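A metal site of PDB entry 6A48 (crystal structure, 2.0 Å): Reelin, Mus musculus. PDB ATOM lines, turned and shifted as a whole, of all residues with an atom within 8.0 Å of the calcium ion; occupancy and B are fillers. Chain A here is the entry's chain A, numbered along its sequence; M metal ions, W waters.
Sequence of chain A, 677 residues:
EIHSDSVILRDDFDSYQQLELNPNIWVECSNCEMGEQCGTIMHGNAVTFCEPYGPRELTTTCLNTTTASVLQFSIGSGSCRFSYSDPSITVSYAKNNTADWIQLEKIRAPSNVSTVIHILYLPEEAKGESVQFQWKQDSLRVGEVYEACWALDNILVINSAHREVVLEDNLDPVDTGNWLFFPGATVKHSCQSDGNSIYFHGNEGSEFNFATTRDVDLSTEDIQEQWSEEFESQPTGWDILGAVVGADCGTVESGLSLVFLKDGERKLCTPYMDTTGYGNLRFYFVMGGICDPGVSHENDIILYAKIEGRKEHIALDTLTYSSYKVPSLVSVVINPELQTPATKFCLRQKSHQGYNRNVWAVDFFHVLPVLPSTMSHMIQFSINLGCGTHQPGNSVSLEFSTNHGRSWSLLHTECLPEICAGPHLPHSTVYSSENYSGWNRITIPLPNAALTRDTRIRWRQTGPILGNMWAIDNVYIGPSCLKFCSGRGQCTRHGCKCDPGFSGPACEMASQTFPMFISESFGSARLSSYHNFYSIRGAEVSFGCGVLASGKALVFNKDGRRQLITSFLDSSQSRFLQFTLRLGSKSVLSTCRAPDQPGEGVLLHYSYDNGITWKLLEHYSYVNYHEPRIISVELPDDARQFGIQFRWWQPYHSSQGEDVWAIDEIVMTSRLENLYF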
ATOM      1  N   GLU A 229      11.209 -10.307  27.607  1.00  0.00           N
ATOM      2  CA  GLU A 229      12.364 -10.222  26.716  1.00  0.00           C
ATOM      3  C   GLU A 229      11.955 -10.770  25.359  1.00  0.00           C
ATOM      4  O   GLU A 229      11.504 -11.919  25.263  1.00  0.00           O
ATOM      5  CB  GLU A 229      13.553 -11.001  27.285  1.00  0.00           C
ATOM      6  CG  GLU A 229      14.751 -11.080  26.328  1.00  0.00           C
ATOM      7  CD  GLU A 229      15.228  -9.715  25.853  1.00  0.00           C
ATOM      8  OE1 GLU A 229      15.356  -8.799  26.686  1.00  0.00           O
ATOM      9  OE2 GLU A 229      15.450  -9.557  24.637  1.00  0.00           O
ATOM     10  N   GLU A 230      12.089  -9.949  24.308  1.00  0.00           N
ATOM     11  CA  GLU A 230      11.625 -10.336  22.983  1.00  0.00           C
ATOM     12  C   GLU A 230      12.730 -10.828  22.064  1.00  0.00           C
ATOM     13  O   GLU A 230      12.430 -11.324  20.979  1.00  0.00           O
ATOM     14  CB  GLU A 230      10.884  -9.172  22.316  1.00  0.00           C
ATOM     15  CG  GLU A 230       9.712  -8.652  23.136  1.00  0.00           C
ATOM     16  CD  GLU A 230       8.500  -8.350  22.269  1.00  0.00           C
ATOM     17  OE1 GLU A 230       8.151  -9.184  21.418  1.00  0.00           O
ATOM     18  OE2 GLU A 230       7.897  -7.271  22.455  1.00  0.00           O
ATOM     19  N   PHE A 231      13.988 -10.698  22.469  1.00  0.00           N
ATOM     20  CA  PHE A 231      15.122 -11.241  21.697  1.00  0.00           C
ATOM     21  C   PHE A 231      15.173 -10.673  20.276  1.00  0.00           C
ATOM     22  O   PHE A 231      15.593 -11.368  19.346  1.00  0.00           O
ATOM     23  CB  PHE A 231      15.074 -12.770  21.644  1.00  0.00           C
ATOM     24  CG  PHE A 231      15.029 -13.438  22.988  1.00  0.00           C
ATOM     25  CD1 PHE A 231      16.169 -13.520  23.781  1.00  0.00           C
ATOM     26  CD2 PHE A 231      13.859 -14.014  23.447  1.00  0.00           C
ATOM     27  CE1 PHE A 231      16.122 -14.150  25.020  1.00  0.00           C
ATOM     28  CE2 PHE A 231      13.812 -14.644  24.685  1.00  0.00           C
ATOM     29  CZ  PHE A 231      14.952 -14.706  25.470  1.00  0.00           C
ATOM     30  N   GLU A 232      14.765  -9.409  20.087  1.00  0.00           N
ATOM     31  CA  GLU A 232      14.981  -8.788  18.783  1.00  0.00           C
ATOM     32  C   GLU A 232      16.433  -8.383  18.577  1.00  0.00           C
ATOM     33  O   GLU A 232      16.797  -7.929  17.490  1.00  0.00           O
ATOM     34  CB  GLU A 232      14.058  -7.571  18.623  1.00  0.00           C
ATOM     35  CG  GLU A 232      12.577  -7.906  18.739  1.00  0.00           C
ATOM     36  CD  GLU A 232      12.129  -8.989  17.758  1.00  0.00           C
ATOM     37  OE1 GLU A 232      12.712  -9.091  16.659  1.00  0.00           O
ATOM     38  OE2 GLU A 232      11.205  -9.751  18.107  1.00  0.00           O
ATOM     39  N   SER A 233      17.256  -8.542  19.612  1.00  0.00           N
ATOM     40  CA  SER A 233      18.703  -8.442  19.557  1.00  0.00           C
ATOM     41  C   SER A 233      19.194  -9.204  20.769  1.00  0.00           C
ATOM     42  O   SER A 233      18.441  -9.423  21.721  1.00  0.00           O
ATOM     43  CB  SER A 233      19.180  -6.987  19.573  1.00  0.00           C
ATOM     44  OG  SER A 233      18.736  -6.330  20.746  1.00  0.00           O
ATOM     45  N   VAL A 245      20.695 -14.876  17.122  1.00  0.00           N
ATOM     46  CA  VAL A 245      19.427 -14.166  17.008  1.00  0.00           C
ATOM     47  C   VAL A 245      18.955 -14.302  15.564  1.00  0.00           C
ATOM     48  O   VAL A 245      19.592 -13.788  14.654  1.00  0.00           O
ATOM     49  CB  VAL A 245      19.559 -12.698  17.420  1.00  0.00           C
ATOM     50  CG1 VAL A 245      18.216 -11.991  17.349  1.00  0.00           C
ATOM     51  CG2 VAL A 245      20.167 -12.585  18.809  1.00  0.00           C
ATOM     52  N   GLY A 246      17.831 -14.978  15.359  1.00  0.00           N
ATOM     53  CA  GLY A 246      17.365 -15.226  14.019  1.00  0.00           C
ATOM     54  C   GLY A 246      15.965 -15.809  13.991  1.00  0.00           C
ATOM     55  O   GLY A 246      15.205 -15.677  14.947  1.00  0.00           O
ATOM     56  N   THR A 251       8.766 -18.140  12.884  1.00  0.00           N
ATOM     57  CA  THR A 251       8.267 -17.266  13.934  1.00  0.00           C
ATOM     58  C   THR A 251       7.912 -18.110  15.155  1.00  0.00           C
ATOM     59  O   THR A 251       7.009 -18.945  15.099  1.00  0.00           O
ATOM     60  CB  THR A 251       7.059 -16.480  13.424  1.00  0.00           C
ATOM     61  OG1 THR A 251       7.441 -15.722  12.277  1.00  0.00           O
ATOM     62  CG2 THR A 251       6.530 -15.543  14.507  1.00  0.00           C
ATOM     63  N   VAL A 252       8.636 -17.898  16.246  1.00  0.00           N
ATOM     64  CA  VAL A 252       8.342 -18.614  17.489  1.00  0.00           C
ATOM     65  C   VAL A 252       7.264 -17.881  18.278  1.00  0.00           C
ATOM     66  O   VAL A 252       6.367 -18.503  18.849  1.00  0.00           O
ATOM     67  CB  VAL A 252       9.621 -18.802  18.308  1.00  0.00           C
ATOM     68  CG1 VAL A 252       9.352 -19.615  19.553  1.00  0.00           C
ATOM     69  CG2 VAL A 252      10.700 -19.463  17.445  1.00  0.00           C
ATOM     70  N   GLU A 253       7.333 -16.548  18.318  1.00  0.00           N
ATOM     71  CA  GLU A 253       6.265 -15.737  18.889  1.00  0.00           C
ATOM     72  C   GLU A 253       6.017 -14.532  17.993  1.00  0.00           C
ATOM     73  O   GLU A 253       4.949 -14.414  17.395  1.00  0.00           O
ATOM     74  CB  GLU A 253       6.620 -15.303  20.318  1.00  0.00           C
ATOM     75  CG  GLU A 253       5.457 -14.716  21.099  1.00  0.00           C
ATOM     76  CD  GLU A 253       5.313 -13.214  20.887  1.00  0.00           C
ATOM     77  OE1 GLU A 253       6.342 -12.533  20.689  1.00  0.00           O
ATOM     78  OE2 GLU A 253       4.165 -12.719  20.940  1.00  0.00           O
ATOM     79  N   SER A 254       7.009 -13.658  17.883  1.00  0.00           N
ATOM     80  CA  SER A 254       6.987 -12.582  16.905  1.00  0.00           C
ATOM     81  C   SER A 254       8.416 -12.088  16.712  1.00  0.00           C
ATOM     82  O   SER A 254       9.238 -12.191  17.625  1.00  0.00           O
ATOM     83  CB  SER A 254       6.075 -11.429  17.335  1.00  0.00           C
ATOM     84  OG  SER A 254       6.434 -10.926  18.614  1.00  0.00           O
ATOM     85  N   GLY A 255       8.685 -11.566  15.525  1.00  0.00           N
ATOM     86  CA  GLY A 255      10.020 -11.053  15.264  1.00  0.00           C
ATOM     87  C   GLY A 255      11.064 -12.154  15.330  1.00  0.00           C
ATOM     88  O   GLY A 255      10.817 -13.312  14.975  1.00  0.00           O
ATOM     89  N   LEU A 256      12.246 -11.783  15.795  1.00  0.00           N
ATOM     90  CA  LEU A 256      13.347 -12.723  15.868  1.00  0.00           C
ATOM     91  C   LEU A 256      13.267 -13.547  17.150  1.00  0.00           C
ATOM     92  O   LEU A 256      12.507 -13.235  18.074  1.00  0.00           O
ATOM     93  CB  LEU A 256      14.681 -11.981  15.796  1.00  0.00           C
ATOM     94  CG  LEU A 256      14.892 -11.170  14.520  1.00  0.00           C
ATOM     95  CD1 LEU A 256      16.156 -10.323  14.611  1.00  0.00           C
ATOM     96  CD2 LEU A 256      14.946 -12.084  13.311  1.00  0.00           C
ATOM     97  N   SER A 257      14.054 -14.616  17.201  1.00  0.00           N
ATOM     98  CA  SER A 257      14.102 -15.498  18.343  1.00  0.00           C
ATOM     99  C   SER A 257      15.557 -15.870  18.611  1.00  0.00           C
ATOM    100  O   SER A 257      16.445 -15.554  17.817  1.00  0.00           O
ATOM    101  CB  SER A 257      13.244 -16.757  18.124  1.00  0.00           C
ATOM    102  OG  SER A 257      13.634 -17.432  16.949  1.00  0.00           O
ATOM    103  N   LEU A 258      15.794 -16.512  19.750  1.00  0.00           N
ATOM    104  CA  LEU A 258      17.084 -17.127  20.048  1.00  0.00           C
ATOM    105  C   LEU A 258      17.073 -18.543  19.491  1.00  0.00           C
ATOM    106  O   LEU A 258      16.341 -19.403  19.982  1.00  0.00           O
ATOM    107  CB  LEU A 258      17.352 -17.147  21.543  1.00  0.00           C
ATOM    108  CG  LEU A 258      18.182 -16.035  22.173  1.00  0.00           C
ATOM    109  CD1 LEU A 258      18.453 -16.368  23.626  1.00  0.00           C
ATOM    110  CD2 LEU A 258      19.480 -15.833  21.410  1.00  0.00           C
ATOM    111  N   VAL A 362      13.728 -20.275  21.362  1.00  0.00           N
ATOM    112  CA  VAL A 362      12.859 -19.695  22.373  1.00  0.00           C
ATOM    113  C   VAL A 362      12.586 -18.243  22.007  1.00  0.00           C
ATOM    114  O   VAL A 362      13.335 -17.610  21.252  1.00  0.00           O
ATOM    115  CB  VAL A 362      13.452 -19.763  23.803  1.00  0.00           C
ATOM    116  CG1 VAL A 362      13.921 -21.175  24.121  1.00  0.00           C
ATOM    117  CG2 VAL A 362      14.580 -18.763  23.949  1.00  0.00           C
ATOM    118  N   ASP A 363      11.493 -17.711  22.559  1.00  0.00           N
ATOM    119  CA  ASP A 363      11.115 -16.330  22.304  1.00  0.00           C
ATOM    120  C   ASP A 363      10.123 -15.878  23.370  1.00  0.00           C
ATOM    121  O   ASP A 363       9.427 -16.698  23.971  1.00  0.00           O
ATOM    122  CB  ASP A 363      10.516 -16.181  20.893  1.00  0.00           C
ATOM    123  CG  ASP A 363      10.468 -14.744  20.429  1.00  0.00           C
ATOM    124  OD1 ASP A 363      11.151 -13.902  21.037  1.00  0.00           O
ATOM    125  OD2 ASP A 363       9.760 -14.463  19.450  1.00  0.00           O
ATOM    126  N   PHE A 364      10.076 -14.568  23.576  1.00  0.00           N
ATOM    127  CA  PHE A 364       9.103 -13.911  24.459  1.00  0.00           C
ATOM    128  C   PHE A 364       9.094 -14.535  25.855  1.00  0.00           C
ATOM    129  O   PHE A 364       8.085 -15.061  26.344  1.00  0.00           O
ATOM    130  CB  PHE A 364       7.706 -13.943  23.823  1.00  0.00           C
ATOM    131  CG  PHE A 364       6.662 -13.181  24.617  1.00  0.00           C
ATOM    132  CD1 PHE A 364       6.955 -11.956  25.182  1.00  0.00           C
ATOM    133  CD2 PHE A 364       5.385 -13.702  24.770  1.00  0.00           C
ATOM    134  CE1 PHE A 364       5.988 -11.260  25.906  1.00  0.00           C
ATOM    135  CE2 PHE A 364       4.414 -13.014  25.498  1.00  0.00           C
ATOM    136  CZ  PHE A 364       4.719 -11.784  26.063  1.00  0.00           C
ATOM    137  N   PHE A 365      10.257 -14.474  26.505  1.00  0.00           N
ATOM    138  CA  PHE A 365      10.305 -14.721  27.949  1.00  0.00           C
ATOM    139  C   PHE A 365       9.477 -13.664  28.666  1.00  0.00           C
ATOM    140  O   PHE A 365       9.599 -12.477  28.381  1.00  0.00           O
ATOM    141  CB  PHE A 365      11.754 -14.676  28.456  1.00  0.00           C
ATOM    142  CG  PHE A 365      12.378 -16.027  28.643  1.00  0.00           C
ATOM    143  CD1 PHE A 365      12.660 -16.830  27.548  1.00  0.00           C
ATOM    144  CD2 PHE A 365      12.698 -16.485  29.905  1.00  0.00           C
ATOM    145  CE1 PHE A 365      13.245 -18.084  27.708  1.00  0.00           C
ATOM    146  CE2 PHE A 365      13.288 -17.735  30.087  1.00  0.00           C
ATOM    147  CZ  PHE A 365      13.553 -18.530  28.985  1.00  0.00           C
HETATM  148 CA    CA M   1      10.874 -12.053  19.324  1.00  0.00          CA
HETATM  149  O   HOH W   1       8.828 -11.586  20.487  1.00  0.00           O
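OD2 of Asp 363 sits close to N of Glu 253, at 3.4 Å.
The side-chain hydroxyl (OG) of Ser 254 lies within hydrogen-bond range of the side-chain carboxylate (OE1) of Glu 253.
C of Gly 255 touches the calcium ion (3.9998 Å).
Within 4 Å of the calcium ion: Glu 230, Glu 232, Ser 254, Gly 255, Leu 256 and Asp 363.
Along chain A the residues within 4 Å of the calcium ion span positions 230 to 363.
The nearest printed residue that does not touch the calcium ion is Ser 257 (4.6 Å).
The calcium ion is bound by the backbone carbonyl oxygen (O) of Ser 254 (2.4 Å), the backbone carbonyl oxygen (O) of Leu 256 (2.4 Å), the backbone carbonyl oxygen (O) of Glu 230 (2.4 Å), water W1 (2.4 Å), the side-chain carboxylate (OD1) of Asp 363 (2.5 Å), the side-chain carboxylate (OE2) of Glu 232 (2.6 Å) and the side-chain carboxylate (OD2) of Asp 363 (2.7 Å).
The calcium ion has seven donor atoms within binding distance.
Water W1 lies within hydrogen-bond range of OE1 of Glu 230 (2.7 Å), OE1 of Glu 253 (2.7 Å) and OG of Ser 254 (3.1 Å).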
